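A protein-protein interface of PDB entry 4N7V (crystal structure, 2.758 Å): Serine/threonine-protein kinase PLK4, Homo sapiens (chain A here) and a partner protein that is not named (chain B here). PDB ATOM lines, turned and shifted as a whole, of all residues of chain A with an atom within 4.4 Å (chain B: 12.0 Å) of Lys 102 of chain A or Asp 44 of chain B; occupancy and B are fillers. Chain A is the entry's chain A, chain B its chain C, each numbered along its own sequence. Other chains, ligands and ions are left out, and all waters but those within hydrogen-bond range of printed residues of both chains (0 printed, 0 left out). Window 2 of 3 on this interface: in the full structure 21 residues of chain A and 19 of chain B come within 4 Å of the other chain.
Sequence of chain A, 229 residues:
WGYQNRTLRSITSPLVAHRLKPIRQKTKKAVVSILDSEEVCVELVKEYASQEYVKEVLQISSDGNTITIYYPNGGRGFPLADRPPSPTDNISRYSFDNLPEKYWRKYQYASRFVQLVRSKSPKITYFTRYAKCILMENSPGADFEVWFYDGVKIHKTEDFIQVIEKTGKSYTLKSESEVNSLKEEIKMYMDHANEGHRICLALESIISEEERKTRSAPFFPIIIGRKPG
Printed residues of chain A that touch a printed residue of chain B: Leu 44, Glu 56, Glu 101, Lys 102 and Lys 106.
Hydrophobic or aromatic side chains of chain A within 4 Å of the printed part of chain B: Leu 44.
Among the printed residues, merely in contact across the chains: Glu 56 of chain A with Asp 44 of chain B, Glu 101 of chain A with Ser 47 of chain B, Glu 101 of chain A with Leu 46 of chain B, Leu 44 of chain A with Asp 44 of chain B and Lys 106 of chain A with Leu 42 of chain B.
The side-chain amino group (NZ) of Lys 106 of chain A lies within salt-bridge range of the side-chain carboxylate (OD1) of Asp 44 of chain B, at 2.6 Å.
The side-chain amino group of Lys 102 of chain A lies within salt-bridge range of the side-chain carboxylate of Asp 44 of chain B (2.8 Å).
Of the printed residues of chain B, Leu 44 of chain A touches Asp 44.
Of the printed residues of chain B, Glu 56 of chain A touches Asp 44 (3.5 Å).
Of chain B, only Leu 46 and Ser 47 come within 4 Å of Glu 101 of chain A.
No residue of chain B comes within 4 Å of Tyr 103 of chain A.
His 39 of chain B touches none of the printed residues of chain A.
Printed residues of chain A within 4 Å of Leu 42 of chain B: Lys 106 (3.9 Å).
Asp 44 of chain B touches just these residues of chain A: Leu 44, Glu 56, Lys 102 and Lys 106.
Printed residues of chain A within 4 Å of Leu 46 of chain B: Glu 101 (3.8 Å).
Of the printed residues of chain A, Ser 47 of chain B touches Glu 101 (3.6 Å).
The nearest residue of chain B that does not touch Lys 102 of chain A is Leu 46 of chain B (4.5 Å).
The side-chain carboxylate (OE2) of Glu 56 of chain A lies within salt-bridge range of the side-chain amino group (NZ) of Lys 106 of chain A, at 3.2 Å.
OH of Tyr 71 of chain A sits at hydrogen-bond distance from OE2 of Glu 56 of chain A (3.3 Å).
The backbone NH (N) of Leu 44 of chain A is in hydrogen-bond range of the backbone carbonyl oxygen (O) of Glu 56 of chain A (2.8 Å).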
ATOM      1  N   LEU A  44       9.406  -6.131 -18.874  1.00  0.00           N
ATOM      2  CA  LEU A  44       9.440  -4.791 -19.460  1.00  0.00           C
ATOM      3  C   LEU A  44      10.002  -3.772 -18.469  1.00  0.00           C
ATOM      4  O   LEU A  44       9.646  -3.781 -17.292  1.00  0.00           O
ATOM      5  CB  LEU A  44       8.049  -4.365 -19.941  1.00  0.00           C
ATOM      6  CG  LEU A  44       7.645  -4.803 -21.354  1.00  0.00           C
ATOM      7  CD1 LEU A  44       7.516  -6.318 -21.477  1.00  0.00           C
ATOM      8  CD2 LEU A  44       6.356  -4.116 -21.779  1.00  0.00           C
ATOM      9  N   GLU A  56       5.859  -4.604 -16.326  1.00  0.00           N
ATOM     10  CA  GLU A  56       5.163  -5.822 -16.719  1.00  0.00           C
ATOM     11  C   GLU A  56       6.112  -7.017 -16.772  1.00  0.00           C
ATOM     12  O   GLU A  56       7.237  -6.901 -17.258  1.00  0.00           O
ATOM     13  CB  GLU A  56       4.499  -5.617 -18.082  1.00  0.00           C
ATOM     14  CG  GLU A  56       3.723  -6.817 -18.593  1.00  0.00           C
ATOM     15  CD  GLU A  56       3.216  -6.620 -20.010  1.00  0.00           C
ATOM     16  OE1 GLU A  56       3.534  -5.577 -20.619  1.00  0.00           O
ATOM     17  OE2 GLU A  56       2.503  -7.510 -20.516  1.00  0.00           O
ATOM     18  N   TYR A  71       1.160  -7.532 -13.232  1.00  0.00           N
ATOM     19  CA  TYR A  71       1.473  -6.113 -13.158  1.00  0.00           C
ATOM     20  C   TYR A  71       1.567  -5.719 -11.689  1.00  0.00           C
ATOM     21  O   TYR A  71       0.618  -5.917 -10.930  1.00  0.00           O
ATOM     22  CB  TYR A  71       0.387  -5.288 -13.852  1.00  0.00           C
ATOM     23  CG  TYR A  71       0.174  -5.625 -15.314  1.00  0.00           C
ATOM     24  CD1 TYR A  71       0.797  -4.893 -16.315  1.00  0.00           C
ATOM     25  CD2 TYR A  71      -0.659  -6.670 -15.693  1.00  0.00           C
ATOM     26  CE1 TYR A  71       0.601  -5.195 -17.653  1.00  0.00           C
ATOM     27  CE2 TYR A  71      -0.861  -6.979 -17.023  1.00  0.00           C
ATOM     28  CZ  TYR A  71      -0.230  -6.240 -17.997  1.00  0.00           C
ATOM     29  OH  TYR A  71      -0.435  -6.552 -19.320  1.00  0.00           O
ATOM     30  N   PRO A 100      -4.525 -13.960 -24.592  1.00  0.00           N
ATOM     31  CA  PRO A 100      -5.229 -12.844 -25.236  1.00  0.00           C
ATOM     32  C   PRO A 100      -4.517 -12.349 -26.492  1.00  0.00           C
ATOM     33  O   PRO A 100      -3.379 -12.743 -26.735  1.00  0.00           O
ATOM     34  CB  PRO A 100      -5.216 -11.759 -24.156  1.00  0.00           C
ATOM     35  CG  PRO A 100      -5.186 -12.520 -22.873  1.00  0.00           C
ATOM     36  CD  PRO A 100      -4.332 -13.730 -23.149  1.00  0.00           C
ATOM     37  N   GLU A 101      -5.182 -11.506 -27.277  1.00  0.00           N
ATOM     38  CA  GLU A 101      -4.582 -10.942 -28.483  1.00  0.00           C
ATOM     39  C   GLU A 101      -3.404 -10.050 -28.114  1.00  0.00           C
ATOM     40  O   GLU A 101      -2.439  -9.935 -28.870  1.00  0.00           O
ATOM     41  CB  GLU A 101      -5.614 -10.154 -29.293  1.00  0.00           C
ATOM     42  CG  GLU A 101      -5.228  -9.935 -30.754  1.00  0.00           C
ATOM     43  CD  GLU A 101      -5.211  -8.465 -31.154  1.00  0.00           C
ATOM     44  OE1 GLU A 101      -4.993  -7.607 -30.270  1.00  0.00           O
ATOM     45  OE2 GLU A 101      -5.420  -8.170 -32.352  1.00  0.00           O
ATOM     46  N   LYS A 102      -3.493  -9.421 -26.944  1.00  0.00           N
ATOM     47  CA  LYS A 102      -2.373  -8.689 -26.365  1.00  0.00           C
ATOM     48  C   LYS A 102      -1.292  -9.711 -26.023  1.00  0.00           C
ATOM     49  O   LYS A 102      -1.563 -10.910 -26.009  1.00  0.00           O
ATOM     50  CB  LYS A 102      -2.834  -7.951 -25.101  1.00  0.00           C
ATOM     51  CG  LYS A 102      -1.846  -6.943 -24.519  1.00  0.00           C
ATOM     52  CD  LYS A 102      -2.402  -6.308 -23.249  1.00  0.00           C
ATOM     53  CE  LYS A 102      -1.348  -5.501 -22.506  1.00  0.00           C
ATOM     54  NZ  LYS A 102      -0.808  -4.375 -23.320  1.00  0.00           N
ATOM     55  N   TYR A 103      -0.073  -9.240 -25.762  1.00  0.00           N
ATOM     56  CA  TYR A 103       1.071 -10.091 -25.395  1.00  0.00           C
ATOM     57  C   TYR A 103       1.622 -10.939 -26.548  1.00  0.00           C
ATOM     58  O   TYR A 103       2.722 -11.485 -26.444  1.00  0.00           O
ATOM     59  CB  TYR A 103       0.762 -11.005 -24.194  1.00  0.00           C
ATOM     60  CG  TYR A 103      -0.027 -10.368 -23.072  1.00  0.00           C
ATOM     61  CD1 TYR A 103       0.571  -9.473 -22.199  1.00  0.00           C
ATOM     62  CD2 TYR A 103      -1.364 -10.685 -22.868  1.00  0.00           C
ATOM     63  CE1 TYR A 103      -0.138  -8.898 -21.169  1.00  0.00           C
ATOM     64  CE2 TYR A 103      -2.087 -10.110 -21.834  1.00  0.00           C
ATOM     65  CZ  TYR A 103      -1.464  -9.216 -20.987  1.00  0.00           C
ATOM     66  OH  TYR A 103      -2.159  -8.631 -19.953  1.00  0.00           O
ATOM     67  N   TRP A 104       0.861 -11.053 -27.632  1.00  0.00           N
ATOM     68  CA  TRP A 104       1.256 -11.882 -28.769  1.00  0.00           C
ATOM     69  C   TRP A 104       2.569 -11.425 -29.399  1.00  0.00           C
ATOM     70  O   TRP A 104       3.357 -12.245 -29.866  1.00  0.00           O
ATOM     71  CB  TRP A 104       0.149 -11.919 -29.821  1.00  0.00           C
ATOM     72  CG  TRP A 104      -0.938 -12.886 -29.494  1.00  0.00           C
ATOM     73  CD1 TRP A 104      -1.045 -13.641 -28.364  1.00  0.00           C
ATOM     74  CD2 TRP A 104      -2.071 -13.214 -30.306  1.00  0.00           C
ATOM     75  NE1 TRP A 104      -2.177 -14.417 -28.419  1.00  0.00           N
ATOM     76  CE2 TRP A 104      -2.824 -14.174 -29.603  1.00  0.00           C
ATOM     77  CE3 TRP A 104      -2.522 -12.790 -31.561  1.00  0.00           C
ATOM     78  CZ2 TRP A 104      -4.004 -14.717 -30.109  1.00  0.00           C
ATOM     79  CZ3 TRP A 104      -3.692 -13.330 -32.063  1.00  0.00           C
ATOM     80  CH2 TRP A 104      -4.420 -14.283 -31.338  1.00  0.00           C
ATOM     81  N   LYS A 106       4.862 -10.173 -27.696  1.00  0.00           N
ATOM     82  CA  LYS A 106       5.873 -10.437 -26.677  1.00  0.00           C
ATOM     83  C   LYS A 106       6.204 -11.924 -26.535  1.00  0.00           C
ATOM     84  O   LYS A 106       7.322 -12.286 -26.166  1.00  0.00           O
ATOM     85  CB  LYS A 106       5.440  -9.842 -25.333  1.00  0.00           C
ATOM     86  CG  LYS A 106       5.131  -8.353 -25.404  1.00  0.00           C
ATOM     87  CD  LYS A 106       4.527  -7.828 -24.109  1.00  0.00           C
ATOM     88  CE  LYS A 106       4.201  -6.340 -24.213  1.00  0.00           C
ATOM     89  NZ  LYS A 106       3.552  -5.806 -22.980  1.00  0.00           N
ATOM     90  N   PRO B  38      14.828  -8.146 -32.585  1.00  0.00           N
ATOM     91  CA  PRO B  38      14.043  -6.936 -32.697  1.00  0.00           C
ATOM     92  C   PRO B  38      13.617  -6.679 -31.279  1.00  0.00           C
ATOM     93  O   PRO B  38      13.008  -7.516 -30.613  1.00  0.00           O
ATOM     94  CB  PRO B  38      12.849  -7.373 -33.540  1.00  0.00           C
ATOM     95  CG  PRO B  38      12.676  -8.815 -33.208  1.00  0.00           C
ATOM     96  CD  PRO B  38      14.061  -9.347 -32.965  1.00  0.00           C
ATOM     97  N   HIS B  39      13.947  -5.484 -30.837  1.00  0.00           N
ATOM     98  CA  HIS B  39      13.492  -4.950 -29.558  1.00  0.00           C
ATOM     99  C   HIS B  39      12.236  -4.096 -29.697  1.00  0.00           C
ATOM    100  O   HIS B  39      11.624  -3.715 -28.699  1.00  0.00           O
ATOM    101  CB  HIS B  39      14.605  -4.142 -28.886  1.00  0.00           C
ATOM    102  CG  HIS B  39      15.735  -4.982 -28.381  1.00  0.00           C
ATOM    103  ND1 HIS B  39      16.474  -5.810 -29.198  1.00  0.00           N
ATOM    104  CD2 HIS B  39      16.251  -5.124 -27.138  1.00  0.00           C
ATOM    105  CE1 HIS B  39      17.397  -6.425 -28.480  1.00  0.00           C
ATOM    106  NE2 HIS B  39      17.283  -6.026 -27.226  1.00  0.00           N
ATOM    107  N   ASP B  40      11.859  -3.796 -30.935  1.00  0.00           N
ATOM    108  CA  ASP B  40      10.643  -3.039 -31.201  1.00  0.00           C
ATOM    109  C   ASP B  40       9.449  -3.963 -31.398  1.00  0.00           C
ATOM    110  O   ASP B  40       8.498  -3.622 -32.099  1.00  0.00           O
ATOM    111  CB  ASP B  40      10.814  -2.131 -32.421  1.00  0.00           C
ATOM    112  CG  ASP B  40      11.209  -0.717 -32.043  1.00  0.00           C
ATOM    113  OD1 ASP B  40      11.915  -0.548 -31.026  1.00  0.00           O
ATOM    114  OD2 ASP B  40      10.807   0.226 -32.759  1.00  0.00           O
ATOM    115  N   MET B  41       9.511  -5.140 -30.784  1.00  0.00           N
ATOM    116  CA  MET B  41       8.372  -6.046 -30.772  1.00  0.00           C
ATOM    117  C   MET B  41       7.796  -6.111 -29.362  1.00  0.00           C
ATOM    118  O   MET B  41       6.721  -6.668 -29.138  1.00  0.00           O
ATOM    119  CB  MET B  41       8.770  -7.440 -31.256  1.00  0.00           C
ATOM    120  CG  MET B  41       7.765  -8.055 -32.222  1.00  0.00           C
ATOM    121  SD  MET B  41       7.887  -9.850 -32.340  1.00  0.00           S
ATOM    122  CE  MET B  41       9.605 -10.045 -32.798  1.00  0.00           C
ATOM    123  N   LEU B  42       8.529  -5.536 -28.415  1.00  0.00           N
ATOM    124  CA  LEU B  42       8.051  -5.404 -27.046  1.00  0.00           C
ATOM    125  C   LEU B  42       7.342  -4.061 -26.890  1.00  0.00           C
ATOM    126  O   LEU B  42       6.985  -3.654 -25.782  1.00  0.00           O
ATOM    127  CB  LEU B  42       9.213  -5.527 -26.060  1.00  0.00           C
ATOM    128  CG  LEU B  42       9.945  -6.872 -26.073  1.00  0.00           C
ATOM    129  CD1 LEU B  42      11.136  -6.841 -25.137  1.00  0.00           C
ATOM    130  CD2 LEU B  42       9.003  -8.007 -25.700  1.00  0.00           C
ATOM    131  N   ASP B  43       7.152  -3.374 -28.015  1.00  0.00           N
ATOM    132  CA  ASP B  43       6.374  -2.143 -28.053  1.00  0.00           C
ATOM    133  C   ASP B  43       4.910  -2.460 -27.787  1.00  0.00           C
ATOM    134  O   ASP B  43       4.373  -3.441 -28.307  1.00  0.00           O
ATOM    135  CB  ASP B  43       6.524  -1.449 -29.407  1.00  0.00           C
ATOM    136  CG  ASP B  43       7.836  -0.697 -29.535  1.00  0.00           C
ATOM    137  OD1 ASP B  43       8.653  -0.753 -28.592  1.00  0.00           O
ATOM    138  OD2 ASP B  43       8.051  -0.054 -30.584  1.00  0.00           O
ATOM    139  N   ASP B  44       4.265  -1.624 -26.981  1.00  0.00           N
ATOM    140  CA  ASP B  44       2.907  -1.905 -26.531  1.00  0.00           C
ATOM    141  C   ASP B  44       1.837  -1.066 -27.232  1.00  0.00           C
ATOM    142  O   ASP B  44       2.132  -0.293 -28.149  1.00  0.00           O
ATOM    143  CB  ASP B  44       2.804  -1.741 -25.012  1.00  0.00           C
ATOM    144  CG  ASP B  44       2.312  -3.000 -24.320  1.00  0.00           C
ATOM    145  OD1 ASP B  44       2.841  -3.338 -23.239  1.00  0.00           O
ATOM    146  OD2 ASP B  44       1.396  -3.656 -24.861  1.00  0.00           O
ATOM    147  N   ASP B  45       0.597  -1.241 -26.779  1.00  0.00           N
ATOM    148  CA  ASP B  45      -0.582  -0.595 -27.357  1.00  0.00           C
ATOM    149  C   ASP B  45      -0.740  -0.896 -28.844  1.00  0.00           C
ATOM    150  O   ASP B  45      -0.252  -0.152 -29.695  1.00  0.00           O
ATOM    151  CB  ASP B  45      -0.577   0.918 -27.112  1.00  0.00           C
ATOM    152  CG  ASP B  45      -1.962   1.460 -26.798  1.00  0.00           C
ATOM    153  OD1 ASP B  45      -2.641   0.887 -25.920  1.00  0.00           O
ATOM    154  OD2 ASP B  45      -2.375   2.457 -27.429  1.00  0.00           O
ATOM    155  N   LEU B  46      -1.427  -1.994 -29.138  1.00  0.00           N
ATOM    156  CA  LEU B  46      -1.734  -2.387 -30.509  1.00  0.00           C
ATOM    157  C   LEU B  46      -3.229  -2.238 -30.799  1.00  0.00           C
ATOM    158  O   LEU B  46      -3.663  -2.345 -31.948  1.00  0.00           O
ATOM    159  CB  LEU B  46      -1.257  -3.822 -30.795  1.00  0.00           C
ATOM    160  CG  LEU B  46      -1.250  -4.931 -29.725  1.00  0.00           C
ATOM    161  CD1 LEU B  46      -0.031  -4.841 -28.797  1.00  0.00           C
ATOM    162  CD2 LEU B  46      -2.553  -5.010 -28.920  1.00  0.00           C
ATOM    163  N   SER B  47      -3.999  -1.984 -29.742  1.00  0.00           N
ATOM    164  CA  SER B  47      -5.456  -1.826 -29.809  1.00  0.00           C
ATOM    165  C   SER B  47      -6.160  -3.027 -30.437  1.00  0.00           C
ATOM    166  O   SER B  47      -5.578  -4.103 -30.579  1.00  0.00           O
ATOM    167  CB  SER B  47      -5.846  -0.531 -30.534  1.00  0.00           C
ATOM    168  OG  SER B  47      -5.516  -0.587 -31.910  1.00  0.00           O
